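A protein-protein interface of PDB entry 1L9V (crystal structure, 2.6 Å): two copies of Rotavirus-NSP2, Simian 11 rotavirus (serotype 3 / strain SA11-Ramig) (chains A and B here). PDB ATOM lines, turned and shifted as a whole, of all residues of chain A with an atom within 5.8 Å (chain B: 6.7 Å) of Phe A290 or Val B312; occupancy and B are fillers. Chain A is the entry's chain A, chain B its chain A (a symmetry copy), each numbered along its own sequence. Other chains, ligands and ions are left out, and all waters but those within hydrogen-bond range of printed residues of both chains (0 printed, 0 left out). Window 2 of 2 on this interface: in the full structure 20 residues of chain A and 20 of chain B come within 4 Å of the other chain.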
ATOM      1  N   TYR A 231      -6.761  23.768  -9.470  1.00  0.00           N
ATOM      2  CA  TYR A 231      -6.523  22.452 -10.054  1.00  0.00           C
ATOM      3  C   TYR A 231      -5.883  22.417 -11.432  1.00  0.00           C
ATOM      4  O   TYR A 231      -5.180  21.465 -11.763  1.00  0.00           O
ATOM      5  CB  TYR A 231      -7.828  21.662 -10.105  1.00  0.00           C
ATOM      6  CG  TYR A 231      -8.339  21.264  -8.741  1.00  0.00           C
ATOM      7  CD1 TYR A 231      -9.356  21.979  -8.119  1.00  0.00           C
ATOM      8  CD2 TYR A 231      -7.801  20.170  -8.077  1.00  0.00           C
ATOM      9  CE1 TYR A 231      -9.825  21.609  -6.874  1.00  0.00           C
ATOM     10  CE2 TYR A 231      -8.264  19.794  -6.825  1.00  0.00           C
ATOM     11  CZ  TYR A 231      -9.276  20.518  -6.234  1.00  0.00           C
ATOM     12  OH  TYR A 231      -9.737  20.138  -5.003  1.00  0.00           O
ATOM     13  N   SER A 232      -6.128  23.438 -12.242  1.00  0.00           N
ATOM     14  CA  SER A 232      -5.550  23.462 -13.569  1.00  0.00           C
ATOM     15  C   SER A 232      -4.046  23.679 -13.466  1.00  0.00           C
ATOM     16  O   SER A 232      -3.343  23.706 -14.475  1.00  0.00           O
ATOM     17  CB  SER A 232      -6.199  24.562 -14.419  1.00  0.00           C
ATOM     18  OG  SER A 232      -5.892  25.853 -13.927  1.00  0.00           O
ATOM     19  N   VAL A 234      -2.040  22.148 -10.459  1.00  0.00           N
ATOM     20  CA  VAL A 234      -1.369  21.111  -9.664  1.00  0.00           C
ATOM     21  C   VAL A 234      -0.335  20.293 -10.420  1.00  0.00           C
ATOM     22  O   VAL A 234       0.749  20.033  -9.899  1.00  0.00           O
ATOM     23  CB  VAL A 234      -2.377  20.117  -9.004  1.00  0.00           C
ATOM     24  CG1 VAL A 234      -3.270  20.847  -8.031  1.00  0.00           C
ATOM     25  CG2 VAL A 234      -3.210  19.431 -10.056  1.00  0.00           C
ATOM     26  N   ALA A 235      -0.668  19.891 -11.643  1.00  0.00           N
ATOM     27  CA  ALA A 235       0.244  19.104 -12.458  1.00  0.00           C
ATOM     28  C   ALA A 235       1.644  19.716 -12.503  1.00  0.00           C
ATOM     29  O   ALA A 235       2.639  18.999 -12.376  1.00  0.00           O
ATOM     30  CB  ALA A 235      -0.310  18.958 -13.867  1.00  0.00           C
ATOM     31  N   TRP A 266      -4.996  18.076  -0.147  1.00  0.00           N
ATOM     32  CA  TRP A 266      -5.828  17.390  -1.129  1.00  0.00           C
ATOM     33  C   TRP A 266      -5.414  15.912  -1.176  1.00  0.00           C
ATOM     34  O   TRP A 266      -4.223  15.580  -1.189  1.00  0.00           O
ATOM     35  CB  TRP A 266      -5.664  18.018  -2.528  1.00  0.00           C
ATOM     36  CG  TRP A 266      -6.463  17.308  -3.600  1.00  0.00           C
ATOM     37  CD1 TRP A 266      -7.705  16.763  -3.462  1.00  0.00           C
ATOM     38  CD2 TRP A 266      -6.088  17.101  -4.968  1.00  0.00           C
ATOM     39  NE1 TRP A 266      -8.131  16.227  -4.657  1.00  0.00           N
ATOM     40  CE2 TRP A 266      -7.160  16.421  -5.599  1.00  0.00           C
ATOM     41  CE3 TRP A 266      -4.951  17.424  -5.726  1.00  0.00           C
ATOM     42  CZ2 TRP A 266      -7.134  16.058  -6.952  1.00  0.00           C
ATOM     43  CZ3 TRP A 266      -4.919  17.058  -7.089  1.00  0.00           C
ATOM     44  CH2 TRP A 266      -6.011  16.382  -7.681  1.00  0.00           C
ATOM     45  N   ASN A 268      -5.249  13.431  -3.488  1.00  0.00           N
ATOM     46  CA  ASN A 268      -4.251  13.062  -4.489  1.00  0.00           C
ATOM     47  C   ASN A 268      -2.871  13.615  -4.196  1.00  0.00           C
ATOM     48  O   ASN A 268      -1.870  12.932  -4.401  1.00  0.00           O
ATOM     49  CB  ASN A 268      -4.693  13.525  -5.873  1.00  0.00           C
ATOM     50  CG  ASN A 268      -5.857  12.728  -6.396  1.00  0.00           C
ATOM     51  OD1 ASN A 268      -6.879  12.587  -5.724  1.00  0.00           O
ATOM     52  ND2 ASN A 268      -5.715  12.198  -7.605  1.00  0.00           N
ATOM     53  N   LYS A 286       3.408  10.820 -10.151  1.00  0.00           N
ATOM     54  CA  LYS A 286       2.535  11.528 -11.086  1.00  0.00           C
ATOM     55  C   LYS A 286       1.175  10.850 -11.318  1.00  0.00           C
ATOM     56  O   LYS A 286       0.132  11.486 -11.189  1.00  0.00           O
ATOM     57  CB  LYS A 286       3.252  11.662 -12.426  1.00  0.00           C
ATOM     58  CG  LYS A 286       2.882  12.878 -13.248  1.00  0.00           C
ATOM     59  CD  LYS A 286       3.755  14.062 -12.878  1.00  0.00           C
ATOM     60  CE  LYS A 286       3.870  15.045 -14.040  1.00  0.00           C
ATOM     61  NZ  LYS A 286       2.581  15.698 -14.427  1.00  0.00           N
ATOM     62  N   ARG A 287       1.190   9.566 -11.670  1.00  0.00           N
ATOM     63  CA  ARG A 287      -0.045   8.823 -11.937  1.00  0.00           C
ATOM     64  C   ARG A 287      -1.100   8.935 -10.845  1.00  0.00           C
ATOM     65  O   ARG A 287      -2.302   8.972 -11.125  1.00  0.00           O
ATOM     66  CB  ARG A 287       0.265   7.342 -12.169  1.00  0.00           C
ATOM     67  CG  ARG A 287       0.970   7.052 -13.472  1.00  0.00           C
ATOM     68  CD  ARG A 287       1.404   5.608 -13.521  1.00  0.00           C
ATOM     69  NE  ARG A 287       2.504   5.410 -14.458  1.00  0.00           N
ATOM     70  CZ  ARG A 287       3.424   4.461 -14.321  1.00  0.00           C
ATOM     71  NH1 ARG A 287       3.363   3.632 -13.287  1.00  0.00           N
ATOM     72  NH2 ARG A 287       4.411   4.352 -15.203  1.00  0.00           N
ATOM     73  N   LEU A 288      -0.650   8.976  -9.598  1.00  0.00           N
ATOM     74  CA  LEU A 288      -1.561   9.069  -8.469  1.00  0.00           C
ATOM     75  C   LEU A 288      -2.334  10.382  -8.463  1.00  0.00           C
ATOM     76  O   LEU A 288      -3.398  10.483  -7.853  1.00  0.00           O
ATOM     77  CB  LEU A 288      -0.782   8.902  -7.164  1.00  0.00           C
ATOM     78  CG  LEU A 288      -0.066   7.554  -7.051  1.00  0.00           C
ATOM     79  CD1 LEU A 288       0.652   7.464  -5.725  1.00  0.00           C
ATOM     80  CD2 LEU A 288      -1.078   6.421  -7.180  1.00  0.00           C
ATOM     81  N   LEU A 289      -1.797  11.382  -9.154  1.00  0.00           N
ATOM     82  CA  LEU A 289      -2.434  12.692  -9.237  1.00  0.00           C
ATOM     83  C   LEU A 289      -3.722  12.625 -10.065  1.00  0.00           C
ATOM     84  O   LEU A 289      -4.688  13.334  -9.771  1.00  0.00           O
ATOM     85  CB  LEU A 289      -1.464  13.698  -9.874  1.00  0.00           C
ATOM     86  CG  LEU A 289      -1.365  15.138  -9.362  1.00  0.00           C
ATOM     87  CD1 LEU A 289      -0.793  15.147  -7.956  1.00  0.00           C
ATOM     88  CD2 LEU A 289      -0.470  15.931 -10.289  1.00  0.00           C
ATOM     89  N   PHE A 290      -3.736  11.763 -11.084  1.00  0.00           N
ATOM     90  CA  PHE A 290      -4.894  11.624 -11.971  1.00  0.00           C
ATOM     91  C   PHE A 290      -5.851  10.475 -11.658  1.00  0.00           C
ATOM     92  O   PHE A 290      -7.011  10.494 -12.071  1.00  0.00           O
ATOM     93  CB  PHE A 290      -4.430  11.493 -13.424  1.00  0.00           C
ATOM     94  CG  PHE A 290      -3.384  12.493 -13.816  1.00  0.00           C
ATOM     95  CD1 PHE A 290      -2.030  12.182 -13.701  1.00  0.00           C
ATOM     96  CD2 PHE A 290      -3.748  13.764 -14.264  1.00  0.00           C
ATOM     97  CE1 PHE A 290      -1.054  13.121 -14.027  1.00  0.00           C
ATOM     98  CE2 PHE A 290      -2.784  14.709 -14.591  1.00  0.00           C
ATOM     99  CZ  PHE A 290      -1.431  14.389 -14.474  1.00  0.00           C
ATOM    100  N   GLN A 291      -5.373   9.468 -10.939  1.00  0.00           N
ATOM    101  CA  GLN A 291      -6.221   8.334 -10.599  1.00  0.00           C
ATOM    102  C   GLN A 291      -7.319   8.752  -9.629  1.00  0.00           C
ATOM    103  O   GLN A 291      -7.040   9.042  -8.466  1.00  0.00           O
ATOM    104  CB  GLN A 291      -5.381   7.221  -9.971  1.00  0.00           C
ATOM    105  CG  GLN A 291      -6.182   5.997  -9.560  1.00  0.00           C
ATOM    106  CD  GLN A 291      -5.332   4.961  -8.858  1.00  0.00           C
ATOM    107  OE1 GLN A 291      -4.389   4.419  -9.435  1.00  0.00           O
ATOM    108  NE2 GLN A 291      -5.661   4.681  -7.604  1.00  0.00           N
ATOM    109  N   LYS A 292      -8.563   8.786 -10.103  1.00  0.00           N
ATOM    110  CA  LYS A 292      -9.678   9.158  -9.238  1.00  0.00           C
ATOM    111  C   LYS A 292      -9.748   8.158  -8.089  1.00  0.00           C
ATOM    112  O   LYS A 292      -9.422   6.984  -8.258  1.00  0.00           O
ATOM    113  CB  LYS A 292     -11.004   9.137 -10.002  1.00  0.00           C
ATOM    114  CG  LYS A 292     -12.159   9.736  -9.202  1.00  0.00           C
ATOM    115  CD  LYS A 292     -13.519   9.441  -9.822  1.00  0.00           C
ATOM    116  CE  LYS A 292     -13.926   7.987  -9.617  1.00  0.00           C
ATOM    117  NZ  LYS A 292     -15.278   7.697 -10.175  1.00  0.00           N
ATOM    118  N   ARG B 307     -15.367  16.898 -12.855  1.00  0.00           N
ATOM    119  CA  ARG B 307     -14.908  18.184 -13.359  1.00  0.00           C
ATOM    120  C   ARG B 307     -13.524  18.509 -12.786  1.00  0.00           C
ATOM    121  O   ARG B 307     -12.599  18.889 -13.513  1.00  0.00           O
ATOM    122  CB  ARG B 307     -15.915  19.275 -12.995  1.00  0.00           C
ATOM    123  CG  ARG B 307     -15.515  20.645 -13.493  1.00  0.00           C
ATOM    124  CD  ARG B 307     -15.051  20.597 -14.944  1.00  0.00           C
ATOM    125  NE  ARG B 307     -14.752  21.931 -15.458  1.00  0.00           N
ATOM    126  CZ  ARG B 307     -15.664  22.888 -15.626  1.00  0.00           C
ATOM    127  NH1 ARG B 307     -16.940  22.657 -15.321  1.00  0.00           N
ATOM    128  NH2 ARG B 307     -15.302  24.073 -16.101  1.00  0.00           N
ATOM    129  N   LYS B 308     -13.391  18.336 -11.475  1.00  0.00           N
ATOM    130  CA  LYS B 308     -12.133  18.570 -10.787  1.00  0.00           C
ATOM    131  C   LYS B 308     -11.038  17.765 -11.484  1.00  0.00           C
ATOM    132  O   LYS B 308      -9.993  18.312 -11.867  1.00  0.00           O
ATOM    133  CB  LYS B 308     -12.253  18.139  -9.324  1.00  0.00           C
ATOM    134  CG  LYS B 308     -10.987  18.302  -8.508  1.00  0.00           C
ATOM    135  CD  LYS B 308     -11.134  17.681  -7.120  1.00  0.00           C
ATOM    136  CE  LYS B 308     -12.210  18.378  -6.276  1.00  0.00           C
ATOM    137  NZ  LYS B 308     -12.225  17.877  -4.865  1.00  0.00           N
ATOM    138  N   MET B 309     -11.280  16.466 -11.661  1.00  0.00           N
ATOM    139  CA  MET B 309     -10.296  15.605 -12.314  1.00  0.00           C
ATOM    140  C   MET B 309      -9.929  16.096 -13.708  1.00  0.00           C
ATOM    141  O   MET B 309      -8.761  16.053 -14.092  1.00  0.00           O
ATOM    142  CB  MET B 309     -10.807  14.166 -12.380  1.00  0.00           C
ATOM    143  CG  MET B 309     -10.886  13.492 -11.022  1.00  0.00           C
ATOM    144  SD  MET B 309      -9.369  13.742 -10.074  1.00  0.00           S
ATOM    145  CE  MET B 309      -8.159  13.151 -11.240  1.00  0.00           C
ATOM    146  N   ASP B 310     -10.919  16.570 -14.464  1.00  0.00           N
ATOM    147  CA  ASP B 310     -10.662  17.074 -15.808  1.00  0.00           C
ATOM    148  C   ASP B 310      -9.723  18.284 -15.745  1.00  0.00           C
ATOM    149  O   ASP B 310      -8.879  18.483 -16.624  1.00  0.00           O
ATOM    150  CB  ASP B 310     -11.973  17.460 -16.506  1.00  0.00           C
ATOM    151  CG  ASP B 310     -12.901  16.278 -16.702  1.00  0.00           C
ATOM    152  OD1 ASP B 310     -12.403  15.137 -16.797  1.00  0.00           O
ATOM    153  OD2 ASP B 310     -14.129  16.488 -16.781  1.00  0.00           O
ATOM    154  N   GLU B 311      -9.875  19.090 -14.698  1.00  0.00           N
ATOM    155  CA  GLU B 311      -9.032  20.258 -14.510  1.00  0.00           C
ATOM    156  C   GLU B 311      -7.601  19.804 -14.248  1.00  0.00           C
ATOM    157  O   GLU B 311      -6.656  20.317 -14.850  1.00  0.00           O
ATOM    158  CB  GLU B 311      -9.527  21.089 -13.324  1.00  0.00           C
ATOM    159  CG  GLU B 311     -10.883  21.755 -13.520  1.00  0.00           C
ATOM    160  CD  GLU B 311     -10.823  22.937 -14.464  1.00  0.00           C
ATOM    161  OE1 GLU B 311      -9.777  23.628 -14.478  1.00  0.00           O
ATOM    162  OE2 GLU B 311     -11.824  23.189 -15.178  1.00  0.00           O
ATOM    163  N   VAL B 312      -7.442  18.838 -13.350  1.00  0.00           N
ATOM    164  CA  VAL B 312      -6.116  18.331 -13.020  1.00  0.00           C
ATOM    165  C   VAL B 312      -5.341  17.945 -14.276  1.00  0.00           C
ATOM    166  O   VAL B 312      -4.106  17.930 -14.261  1.00  0.00           O
ATOM    167  CB  VAL B 312      -6.193  17.110 -12.074  1.00  0.00           C
ATOM    168  CG1 VAL B 312      -4.793  16.615 -11.740  1.00  0.00           C
ATOM    169  CG2 VAL B 312      -6.925  17.492 -10.798  1.00  0.00           C
ATOM    170  N   SER B 313      -6.058  17.650 -15.361  1.00  0.00           N
ATOM    171  CA  SER B 313      -5.416  17.276 -16.626  1.00  0.00           C
ATOM    172  C   SER B 313      -5.723  18.220 -17.797  1.00  0.00           C
ATOM    173  O   SER B 313      -6.648  19.047 -17.684  1.00  0.00           O
ATOM    174  CB  SER B 313      -5.818  15.851 -17.002  1.00  0.00           C
ATOM    175  OG  SER B 313      -7.225  15.734 -17.078  1.00  0.00           O
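No position is printed for both chains.
Of the 7 printed residues of chain B, 4 touch a printed residue of chain A. Printed residues of chain B that touch a printed residue of chain A: Lys B308, Met B309, Glu B311 and Val B312. Of the 13 printed residues of chain A, 7 touch a printed residue of chain B. Among the printed residues, 11 pairs touch across the chains.
O of Tyr A231 touches O of Glu B311, at 3.6 Å. Val B312 touches Tyr A231 (CA to O, 3.5 Å). CA of Ser A232 touches O of Glu B311, 3.6 Å away. CG2 of Val A234 touches CG1 of Val B312, at 3.6 Å. Ala A235 touches Val B312 (CB to O, 3.95 Å). CH2 of Trp A266 touches CG2 of Val B312 (3.4 Å). Leu A289 touches Met B309. CG1 of Val B312 touches O of Leu A289 (3.8 Å). Met B309 touches Phe A290. Val B312 touches Phe A290 (O to CE2, 3.5 Å).
The side-chain amide nitrogen (ND2) of Asn A268 lies within hydrogen-bond range of the backbone carbonyl oxygen (O) of Leu A289. OE2 of Glu B311 is in salt-bridge range of NE of Arg B307 (3.2 Å). O of Met B309 sits at hydrogen-bond distance from OG of Ser B313 (3.4 Å).
Lys A286 touches none of the printed residues of chain B. Of the printed residues of chain B, Phe A290 touches Met B309 (3.0 Å) and Val B312 (3.5 Å). Arg B307 touches none of the printed residues of chain A. Of the printed residues of chain A, Lys B308 touches Tyr A231 (3.3 Å). Printed residues of chain A within 4 Å of Met B309: Leu A289 and Phe A290. Val B312 touches six residues of chain A. The nearest residue of chain A that does not touch Val B312 is Ser A232 (4.9 Å). The nearest printed residue of chain A that does not touch Met B309 is Lys A292 (4.4 Å).
NZ of Lys B308 sits close to OH of Tyr A231 (3.4 Å).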
